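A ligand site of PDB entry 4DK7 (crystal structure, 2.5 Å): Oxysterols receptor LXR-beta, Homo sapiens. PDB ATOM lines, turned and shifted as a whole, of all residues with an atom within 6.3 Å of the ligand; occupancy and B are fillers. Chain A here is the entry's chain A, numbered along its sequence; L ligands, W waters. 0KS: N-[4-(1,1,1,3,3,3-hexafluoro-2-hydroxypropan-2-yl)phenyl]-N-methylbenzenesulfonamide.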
ATOM      1  N   PHE A  54      -4.668   9.696  31.262  1.00  0.00           N
ATOM      2  CA  PHE A  54      -5.607   9.673  30.159  1.00  0.00           C
ATOM      3  C   PHE A  54      -6.400  10.979  30.111  1.00  0.00           C
ATOM      4  O   PHE A  54      -6.536  11.604  29.054  1.00  0.00           O
ATOM      5  CB  PHE A  54      -6.565   8.493  30.310  1.00  0.00           C
ATOM      6  CG  PHE A  54      -7.577   8.394  29.212  1.00  0.00           C
ATOM      7  CD1 PHE A  54      -7.200   7.991  27.948  1.00  0.00           C
ATOM      8  CD2 PHE A  54      -8.903   8.700  29.458  1.00  0.00           C
ATOM      9  CE1 PHE A  54      -8.138   7.884  26.930  1.00  0.00           C
ATOM     10  CE2 PHE A  54      -9.849   8.594  28.445  1.00  0.00           C
ATOM     11  CZ  PHE A  54      -9.472   8.190  27.182  1.00  0.00           C
ATOM     12  N   PHE A  57      -4.226  13.640  28.653  1.00  0.00           N
ATOM     13  CA  PHE A  57      -4.203  13.574  27.200  1.00  0.00           C
ATOM     14  C   PHE A  57      -5.491  14.116  26.598  1.00  0.00           C
ATOM     15  O   PHE A  57      -5.443  14.992  25.730  1.00  0.00           O
ATOM     16  CB  PHE A  57      -3.963  12.143  26.735  1.00  0.00           C
ATOM     17  CG  PHE A  57      -2.523  11.854  26.370  1.00  0.00           C
ATOM     18  CD1 PHE A  57      -2.193  11.441  25.090  1.00  0.00           C
ATOM     19  CD2 PHE A  57      -1.521  12.025  27.298  1.00  0.00           C
ATOM     20  CE1 PHE A  57      -0.869  11.199  24.743  1.00  0.00           C
ATOM     21  CE2 PHE A  57      -0.205  11.784  26.958  1.00  0.00           C
ATOM     22  CZ  PHE A  57       0.125  11.371  25.677  1.00  0.00           C
ATOM     23  N   THR A  58      -6.637  13.612  27.063  1.00  0.00           N
ATOM     24  CA  THR A  58      -7.929  14.032  26.521  1.00  0.00           C
ATOM     25  C   THR A  58      -8.135  15.541  26.644  1.00  0.00           C
ATOM     26  O   THR A  58      -8.766  16.153  25.781  1.00  0.00           O
ATOM     27  CB  THR A  58      -9.113  13.346  27.238  1.00  0.00           C
ATOM     28  OG1 THR A  58      -9.018  13.587  28.655  1.00  0.00           O
ATOM     29  CG2 THR A  58      -9.124  11.849  26.962  1.00  0.00           C
ATOM     30  N   GLU A  59      -7.601  16.133  27.697  1.00  0.00           N
ATOM     31  CA  GLU A  59      -7.714  17.572  27.860  1.00  0.00           C
ATOM     32  C   GLU A  59      -6.808  18.351  26.906  1.00  0.00           C
ATOM     33  O   GLU A  59      -7.189  19.414  26.410  1.00  0.00           O
ATOM     34  CB  GLU A  59      -7.442  17.963  29.317  1.00  0.00           C
ATOM     35  CG  GLU A  59      -8.689  17.886  30.197  1.00  0.00           C
ATOM     36  CD  GLU A  59      -8.350  17.829  31.669  1.00  0.00           C
ATOM     37  OE1 GLU A  59      -7.312  18.386  32.066  1.00  0.00           O
ATOM     38  OE2 GLU A  59      -9.119  17.210  32.432  1.00  0.00           O
ATOM     39  N   LEU A  60      -5.621  17.819  26.632  1.00  0.00           N
ATOM     40  CA  LEU A  60      -4.790  18.389  25.581  1.00  0.00           C
ATOM     41  C   LEU A  60      -5.508  18.248  24.241  1.00  0.00           C
ATOM     42  O   LEU A  60      -5.443  19.130  23.399  1.00  0.00           O
ATOM     43  CB  LEU A  60      -3.432  17.694  25.529  1.00  0.00           C
ATOM     44  CG  LEU A  60      -2.579  17.816  26.803  1.00  0.00           C
ATOM     45  CD1 LEU A  60      -1.311  16.984  26.643  1.00  0.00           C
ATOM     46  CD2 LEU A  60      -2.227  19.265  27.075  1.00  0.00           C
ATOM     47  N   ALA A  61      -6.213  17.140  24.057  1.00  0.00           N
ATOM     48  CA  ALA A  61      -6.888  16.932  22.790  1.00  0.00           C
ATOM     49  C   ALA A  61      -8.028  17.921  22.600  1.00  0.00           C
ATOM     50  O   ALA A  61      -8.249  18.417  21.496  1.00  0.00           O
ATOM     51  CB  ALA A  61      -7.408  15.503  22.717  1.00  0.00           C
ATOM     52  N   ILE A  62      -8.748  18.223  23.693  1.00  0.00           N
ATOM     53  CA  ILE A  62      -9.816  19.217  23.632  1.00  0.00           C
ATOM     54  C   ILE A  62      -9.255  20.570  23.240  1.00  0.00           C
ATOM     55  O   ILE A  62      -9.868  21.303  22.449  1.00  0.00           O
ATOM     56  CB  ILE A  62     -10.508  19.379  25.000  1.00  0.00           C
ATOM     57  CG1 ILE A  62     -11.332  18.121  25.310  1.00  0.00           C
ATOM     58  CG2 ILE A  62     -11.413  20.627  24.986  1.00  0.00           C
ATOM     59  CD1 ILE A  62     -11.893  18.105  26.712  1.00  0.00           C
ATOM     60  N   SER A  64      -6.630  21.137  21.425  1.00  0.00           N
ATOM     61  CA  SER A  64      -6.343  21.062  19.994  1.00  0.00           C
ATOM     62  C   SER A  64      -7.571  21.242  19.128  1.00  0.00           C
ATOM     63  O   SER A  64      -7.532  21.989  18.146  1.00  0.00           O
ATOM     64  CB  SER A  64      -5.673  19.721  19.633  1.00  0.00           C
ATOM     65  OG  SER A  64      -4.277  19.774  19.871  1.00  0.00           O
ATOM     66  N   ILE A  95      -8.593  14.844  13.372  1.00  0.00           N
ATOM     67  CA  ILE A  95      -7.573  13.952  13.885  1.00  0.00           C
ATOM     68  C   ILE A  95      -6.349  14.037  12.987  1.00  0.00           C
ATOM     69  O   ILE A  95      -5.222  13.915  13.433  1.00  0.00           O
ATOM     70  CB  ILE A  95      -8.073  12.498  13.955  1.00  0.00           C
ATOM     71  CG1 ILE A  95      -7.004  11.626  14.616  1.00  0.00           C
ATOM     72  CG2 ILE A  95      -8.419  11.969  12.561  1.00  0.00           C
ATOM     73  CD1 ILE A  95      -6.790  11.975  16.044  1.00  0.00           C
ATOM     74  N   MET A  98      -4.588  17.363  13.822  1.00  0.00           N
ATOM     75  CA  MET A  98      -3.891  17.094  15.072  1.00  0.00           C
ATOM     76  C   MET A  98      -2.571  16.351  14.855  1.00  0.00           C
ATOM     77  O   MET A  98      -1.552  16.649  15.502  1.00  0.00           O
ATOM     78  CB  MET A  98      -4.758  16.244  15.979  1.00  0.00           C
ATOM     79  CG  MET A  98      -5.251  16.974  17.220  1.00  0.00           C
ATOM     80  SD  MET A  98      -6.404  15.857  18.299  1.00  0.00           S
ATOM     81  CE  MET A  98      -7.871  15.867  17.115  1.00  0.00           C
ATOM     82  N   LEU A  99      -2.565  15.369  13.970  1.00  0.00           N
ATOM     83  CA  LEU A  99      -1.369  14.587  13.767  1.00  0.00           C
ATOM     84  C   LEU A  99      -0.284  15.410  13.051  1.00  0.00           C
ATOM     85  O   LEU A  99       0.888  15.310  13.381  1.00  0.00           O
ATOM     86  CB  LEU A  99      -1.717  13.320  12.988  1.00  0.00           C
ATOM     87  CG  LEU A  99      -2.584  12.370  13.812  1.00  0.00           C
ATOM     88  CD1 LEU A  99      -3.386  11.468  12.906  1.00  0.00           C
ATOM     89  CD2 LEU A  99      -1.688  11.565  14.697  1.00  0.00           C
ATOM     90  N   THR A 102       1.055  17.523  15.792  1.00  0.00           N
ATOM     91  CA  THR A 102       1.916  16.725  16.641  1.00  0.00           C
ATOM     92  C   THR A 102       3.287  16.550  15.992  1.00  0.00           C
ATOM     93  O   THR A 102       4.320  16.643  16.661  1.00  0.00           O
ATOM     94  CB  THR A 102       1.307  15.341  16.906  1.00  0.00           C
ATOM     95  OG1 THR A 102       0.057  15.500  17.595  1.00  0.00           O
ATOM     96  CG2 THR A 102       2.243  14.498  17.763  1.00  0.00           C
ATOM     97  N   ARG A 105       5.653  19.256  16.581  1.00  0.00           N
ATOM     98  CA  ARG A 105       6.243  19.380  17.909  1.00  0.00           C
ATOM     99  C   ARG A 105       7.206  18.222  18.226  1.00  0.00           C
ATOM    100  O   ARG A 105       7.643  18.054  19.359  1.00  0.00           O
ATOM    101  CB  ARG A 105       5.140  19.454  18.962  1.00  0.00           C
ATOM    102  CG  ARG A 105       4.204  20.646  18.812  1.00  0.00           C
ATOM    103  CD  ARG A 105       2.902  20.395  19.585  1.00  0.00           C
ATOM    104  NE  ARG A 105       2.196  21.631  19.918  1.00  0.00           N
ATOM    105  CZ  ARG A 105       0.958  21.673  20.415  1.00  0.00           C
ATOM    106  NH1 ARG A 105       0.383  22.840  20.679  1.00  0.00           N
ATOM    107  NH2 ARG A 105       0.294  20.536  20.628  1.00  0.00           N
ATOM    108  N   ILE A 113       7.580  14.283  21.967  1.00  0.00           N
ATOM    109  CA  ILE A 113       6.741  15.345  21.463  1.00  0.00           C
ATOM    110  C   ILE A 113       6.504  16.308  22.618  1.00  0.00           C
ATOM    111  O   ILE A 113       6.167  15.897  23.737  1.00  0.00           O
ATOM    112  CB  ILE A 113       5.418  14.737  20.961  1.00  0.00           C
ATOM    113  CG1 ILE A 113       5.735  13.718  19.861  1.00  0.00           C
ATOM    114  CG2 ILE A 113       4.484  15.839  20.453  1.00  0.00           C
ATOM    115  CD1 ILE A 113       4.598  12.779  19.491  1.00  0.00           C
ATOM    116  N   PHE A 115       4.200  18.865  24.199  1.00  0.00           N
ATOM    117  CA  PHE A 115       2.802  19.279  24.084  1.00  0.00           C
ATOM    118  C   PHE A 115       2.459  20.613  24.730  1.00  0.00           C
ATOM    119  O   PHE A 115       1.449  21.235  24.386  1.00  0.00           O
ATOM    120  CB  PHE A 115       1.881  18.184  24.654  1.00  0.00           C
ATOM    121  CG  PHE A 115       1.600  17.081  23.686  1.00  0.00           C
ATOM    122  CD1 PHE A 115       1.862  15.764  24.021  1.00  0.00           C
ATOM    123  CD2 PHE A 115       1.067  17.358  22.431  1.00  0.00           C
ATOM    124  CE1 PHE A 115       1.606  14.738  23.123  1.00  0.00           C
ATOM    125  CE2 PHE A 115       0.822  16.345  21.530  1.00  0.00           C
ATOM    126  CZ  PHE A 115       1.089  15.032  21.872  1.00  0.00           C
ATOM    127  N   PHE A 126       3.103   8.055  26.458  1.00  0.00           N
ATOM    128  CA  PHE A 126       1.872   7.745  25.742  1.00  0.00           C
ATOM    129  C   PHE A 126       1.318   6.430  26.270  1.00  0.00           C
ATOM    130  O   PHE A 126       0.110   6.263  26.389  1.00  0.00           O
ATOM    131  CB  PHE A 126       2.129   7.611  24.232  1.00  0.00           C
ATOM    132  CG  PHE A 126       2.272   8.923  23.511  1.00  0.00           C
ATOM    133  CD1 PHE A 126       3.228   9.853  23.914  1.00  0.00           C
ATOM    134  CD2 PHE A 126       1.464   9.218  22.418  1.00  0.00           C
ATOM    135  CE1 PHE A 126       3.365  11.053  23.248  1.00  0.00           C
ATOM    136  CE2 PHE A 126       1.594  10.422  21.740  1.00  0.00           C
ATOM    137  CZ  PHE A 126       2.543  11.344  22.153  1.00  0.00           C
ATOM    138  N   LEU A 131      -2.733   4.309  26.104  1.00  0.00           N
ATOM    139  CA  LEU A 131      -2.689   4.114  24.658  1.00  0.00           C
ATOM    140  C   LEU A 131      -1.932   2.856  24.277  1.00  0.00           C
ATOM    141  O   LEU A 131      -1.016   2.433  24.994  1.00  0.00           O
ATOM    142  CB  LEU A 131      -2.056   5.319  23.984  1.00  0.00           C
ATOM    143  CG  LEU A 131      -2.851   6.616  24.098  1.00  0.00           C
ATOM    144  CD1 LEU A 131      -2.251   7.678  23.184  1.00  0.00           C
ATOM    145  CD2 LEU A 131      -4.305   6.323  23.718  1.00  0.00           C
ATOM    146  N   PHE A 135      -1.010   2.128  17.944  1.00  0.00           N
ATOM    147  CA  PHE A 135      -1.354   3.494  17.589  1.00  0.00           C
ATOM    148  C   PHE A 135      -0.125   4.369  17.829  1.00  0.00           C
ATOM    149  O   PHE A 135       0.253   5.195  16.979  1.00  0.00           O
ATOM    150  CB  PHE A 135      -2.535   3.980  18.450  1.00  0.00           C
ATOM    151  CG  PHE A 135      -2.966   5.400  18.158  1.00  0.00           C
ATOM    152  CD1 PHE A 135      -2.875   5.912  16.871  1.00  0.00           C
ATOM    153  CD2 PHE A 135      -3.475   6.202  19.164  1.00  0.00           C
ATOM    154  CE1 PHE A 135      -3.291   7.217  16.594  1.00  0.00           C
ATOM    155  CE2 PHE A 135      -3.889   7.498  18.891  1.00  0.00           C
ATOM    156  CZ  PHE A 135      -3.798   8.010  17.604  1.00  0.00           C
ATOM    157  N   ILE A 139       2.134   6.973  15.106  1.00  0.00           N
ATOM    158  CA  ILE A 139       2.220   8.418  15.354  1.00  0.00           C
ATOM    159  C   ILE A 139       3.650   8.928  15.291  1.00  0.00           C
ATOM    160  O   ILE A 139       3.938   9.951  14.672  1.00  0.00           O
ATOM    161  CB  ILE A 139       1.665   8.805  16.749  1.00  0.00           C
ATOM    162  CG1 ILE A 139       0.169   8.499  16.840  1.00  0.00           C
ATOM    163  CG2 ILE A 139       1.894  10.286  17.013  1.00  0.00           C
ATOM    164  CD1 ILE A 139      -0.388   8.720  18.228  1.00  0.00           C
ATOM    165  N   HIS A 221      -6.594   5.482  14.654  1.00  0.00           N
ATOM    166  CA  HIS A 221      -7.106   6.210  15.811  1.00  0.00           C
ATOM    167  C   HIS A 221      -8.512   5.724  16.204  1.00  0.00           C
ATOM    168  O   HIS A 221      -8.798   5.564  17.379  1.00  0.00           O
ATOM    169  CB  HIS A 221      -7.147   7.708  15.507  1.00  0.00           C
ATOM    170  CG  HIS A 221      -7.757   8.522  16.614  1.00  0.00           C
ATOM    171  ND1 HIS A 221      -8.991   9.118  16.497  1.00  0.00           N
ATOM    172  CD2 HIS A 221      -7.311   8.815  17.853  1.00  0.00           C
ATOM    173  CE1 HIS A 221      -9.287   9.731  17.629  1.00  0.00           C
ATOM    174  NE2 HIS A 221      -8.288   9.568  18.471  1.00  0.00           N
ATOM    175  N   GLN A 224      -8.226   2.823  18.132  1.00  0.00           N
ATOM    176  CA  GLN A 224      -7.818   3.169  19.472  1.00  0.00           C
ATOM    177  C   GLN A 224      -9.045   3.562  20.289  1.00  0.00           C
ATOM    178  O   GLN A 224      -9.203   3.129  21.428  1.00  0.00           O
ATOM    179  CB  GLN A 224      -6.803   4.304  19.452  1.00  0.00           C
ATOM    180  CG  GLN A 224      -6.424   4.851  20.840  1.00  0.00           C
ATOM    181  CD  GLN A 224      -5.746   3.820  21.739  1.00  0.00           C
ATOM    182  OE1 GLN A 224      -4.517   3.707  21.788  1.00  0.00           O
ATOM    183  NE2 GLN A 224      -6.559   3.055  22.466  1.00  0.00           N
ATOM    184  N   VAL A 225      -9.920   4.370  19.694  1.00  0.00           N
ATOM    185  CA  VAL A 225     -11.096   4.857  20.397  1.00  0.00           C
ATOM    186  C   VAL A 225     -11.991   3.691  20.789  1.00  0.00           C
ATOM    187  O   VAL A 225     -12.515   3.653  21.902  1.00  0.00           O
ATOM    188  CB  VAL A 225     -11.909   5.836  19.514  1.00  0.00           C
ATOM    189  CG1 VAL A 225     -13.266   6.150  20.154  1.00  0.00           C
ATOM    190  CG2 VAL A 225     -11.114   7.116  19.307  1.00  0.00           C
ATOM    191  N   LEU A 228     -10.689   1.640  23.610  1.00  0.00           N
ATOM    192  CA  LEU A 228     -10.815   2.316  24.889  1.00  0.00           C
ATOM    193  C   LEU A 228     -12.167   2.020  25.532  1.00  0.00           C
ATOM    194  O   LEU A 228     -12.289   2.015  26.766  1.00  0.00           O
ATOM    195  CB  LEU A 228     -10.656   3.818  24.710  1.00  0.00           C
ATOM    196  CG  LEU A 228      -9.248   4.299  24.376  1.00  0.00           C
ATOM    197  CD1 LEU A 228      -9.291   5.771  24.090  1.00  0.00           C
ATOM    198  CD2 LEU A 228      -8.309   3.998  25.524  1.00  0.00           C
ATOM    199  N   LEU A 235     -14.577   8.889  26.063  1.00  0.00           N
ATOM    200  CA  LEU A 235     -14.150  10.234  25.684  1.00  0.00           C
ATOM    201  C   LEU A 235     -15.003  11.302  26.376  1.00  0.00           C
ATOM    202  O   LEU A 235     -16.195  11.123  26.576  1.00  0.00           O
ATOM    203  CB  LEU A 235     -14.249  10.416  24.170  1.00  0.00           C
ATOM    204  CG  LEU A 235     -13.326   9.560  23.311  1.00  0.00           C
ATOM    205  CD1 LEU A 235     -13.619   9.792  21.839  1.00  0.00           C
ATOM    206  CD2 LEU A 235     -11.884   9.889  23.633  1.00  0.00           C
ATOM    207  N   PRO A 236     -14.381  12.436  26.724  1.00  0.00           N
ATOM    208  CA  PRO A 236     -15.138  13.582  27.225  1.00  0.00           C
ATOM    209  C   PRO A 236     -16.111  14.064  26.156  1.00  0.00           C
ATOM    210  O   PRO A 236     -16.019  13.665  24.987  1.00  0.00           O
ATOM    211  CB  PRO A 236     -14.053  14.612  27.526  1.00  0.00           C
ATOM    212  CG  PRO A 236     -12.818  13.795  27.754  1.00  0.00           C
ATOM    213  CD  PRO A 236     -12.929  12.652  26.796  1.00  0.00           C
ATOM    214  N   LEU A 239     -14.889  15.482  22.483  1.00  0.00           N
ATOM    215  CA  LEU A 239     -14.237  14.441  21.700  1.00  0.00           C
ATOM    216  C   LEU A 239     -15.251  13.376  21.292  1.00  0.00           C
ATOM    217  O   LEU A 239     -15.272  12.930  20.135  1.00  0.00           O
ATOM    218  CB  LEU A 239     -13.097  13.812  22.506  1.00  0.00           C
ATOM    219  CG  LEU A 239     -12.085  14.837  23.042  1.00  0.00           C
ATOM    220  CD1 LEU A 239     -10.959  14.123  23.777  1.00  0.00           C
ATOM    221  CD2 LEU A 239     -11.534  15.670  21.887  1.00  0.00           C
ATOM    222  N   TRP A 243     -15.776  11.837  17.677  1.00  0.00           N
ATOM    223  CA  TRP A 243     -15.198  10.556  17.281  1.00  0.00           C
ATOM    224  C   TRP A 243     -16.012   9.308  17.605  1.00  0.00           C
ATOM    225  O   TRP A 243     -15.762   8.240  17.032  1.00  0.00           O
ATOM    226  CB  TRP A 243     -13.796  10.393  17.861  1.00  0.00           C
ATOM    227  CG  TRP A 243     -12.798  11.397  17.344  1.00  0.00           C
ATOM    228  CD1 TRP A 243     -12.613  11.790  16.047  1.00  0.00           C
ATOM    229  CD2 TRP A 243     -11.838  12.126  18.122  1.00  0.00           C
ATOM    230  NE1 TRP A 243     -11.599  12.711  15.969  1.00  0.00           N
ATOM    231  CE2 TRP A 243     -11.109  12.933  17.227  1.00  0.00           C
ATOM    232  CE3 TRP A 243     -11.529  12.156  19.484  1.00  0.00           C
ATOM    233  CZ2 TRP A 243     -10.080  13.770  17.658  1.00  0.00           C
ATOM    234  CZ3 TRP A 243     -10.514  12.989  19.914  1.00  0.00           C
ATOM    235  CH2 TRP A 243      -9.796  13.794  19.000  1.00  0.00           C
HETATM  236  C1  0KS L   1      -6.205  10.661  21.122  1.00  0.00           C
HETATM  237  C2  0KS L   1      -4.936  10.192  21.559  1.00  0.00           C
HETATM  238  C3  0KS L   1      -6.218  11.526  19.994  1.00  0.00           C
HETATM  239  C4  0KS L   1      -3.755  10.570  20.920  1.00  0.00           C
HETATM  240  C5  0KS L   1      -5.047  11.914  19.356  1.00  0.00           C
HETATM  241  C6  0KS L   1      -3.771  11.441  19.805  1.00  0.00           C
HETATM  242  N1  0KS L   1      -2.517  11.791  19.206  1.00  0.00           N
HETATM  243  S2  0KS L   1      -1.337  12.832  20.021  1.00  0.00           S
HETATM  244  O4  0KS L   1      -0.347  13.176  19.033  1.00  0.00           O
HETATM  245  O5  0KS L   1      -0.863  12.052  21.136  1.00  0.00           O
HETATM  246  C8  0KS L   1      -2.120  14.341  20.635  1.00  0.00           C
HETATM  247  C9  0KS L   1      -2.695  14.363  21.938  1.00  0.00           C
HETATM  248  C10 0KS L   1      -2.131  15.504  19.817  1.00  0.00           C
HETATM  249  C11 0KS L   1      -2.733  16.692  20.295  1.00  0.00           C
HETATM  250  C12 0KS L   1      -3.290  15.551  22.410  1.00  0.00           C
HETATM  251  C13 0KS L   1      -3.295  16.699  21.583  1.00  0.00           C
HETATM  252  C7  0KS L   1      -2.804  12.295  17.833  1.00  0.00           C
HETATM  253  C18 0KS L   1      -7.538  10.276  21.785  1.00  0.00           C
HETATM  254  C19 0KS L   1      -7.816  11.193  23.028  1.00  0.00           C
HETATM  255  C20 0KS L   1      -7.609   8.711  22.087  1.00  0.00           C
HETATM  256  F5  0KS L   1      -9.000  10.882  23.622  1.00  0.00           F
HETATM  257  F4  0KS L   1      -7.869  12.510  22.648  1.00  0.00           F
HETATM  258  F6  0KS L   1      -6.856  11.102  23.987  1.00  0.00           F
HETATM  259  F7  0KS L   1      -8.803   8.381  22.647  1.00  0.00           F
HETATM  260  F9  0KS L   1      -6.662   8.296  22.961  1.00  0.00           F
HETATM  261  F8  0KS L   1      -7.434   7.981  20.926  1.00  0.00           F
HETATM  262  O1  0KS L   1      -8.638  10.489  20.893  1.00  0.00           O
HETATM  263  O   HOH W   1      -1.325  19.158  18.867  1.00  0.00           O
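An oxygen (O1) of the ligand lies within hydrogen-bond range of a ring nitrogen (NE2) of His 221 (2.6 Å). An oxygen (O4) of the ligand lies within hydrogen-bond range of the side-chain hydroxyl (OG1) of Thr 102 (2.8 Å).
The backbone carbonyl oxygen (O) of Phe 54 lies within hydrogen-bond range of the side-chain hydroxyl (OG1) of Thr 58 (3.2 Å). OG1 of Thr 102 sits at hydrogen-bond distance from O of Met 98, 2.9 Å away. The backbone NH of Leu 131 sits close to the backbone carbonyl oxygen of Phe 126 (3.5 Å).
Phe 57 touches the ligand. CG2 of Thr 58 touches F5 of the ligand, at 3.5 Å. Leu 60 touches the ligand (O to C13, 3.7 Å). Ala 61 touches the ligand. Ser 64 touches the ligand. CD1 of Ile 95 touches C5 of the ligand (3.7 Å). CG of Met 98 touches C11 of the ligand, 3.98 Å away. CD2 of Leu 99 touches C7 of the ligand, 3.4 Å away. CZ of Phe 115 touches C8 of the ligand, 3.5 Å away. Phe 126 touches the ligand. Leu 131 touches the ligand (CD2 to F9, 3.2 Å). Phe 135 touches the ligand. Ile 139 touches the ligand (CD1 to N1, 3.9 Å). Gln 224 touches the ligand. Leu 228 touches the ligand. Leu 235 touches the ligand. Leu 239 touches the ligand (CD1 to F4, 3.7 Å). Trp 243 touches the ligand. Of the 27 residues printed, 20 come within 4 Å of the ligand. The nearest printed residue that does not touch the ligand is Val 225 (4.1 Å).
Water W1 bridges the guanidinium group of Arg 105 (2.8 Å) and the side-chain hydroxyl of Ser 64 (3.2 Å).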
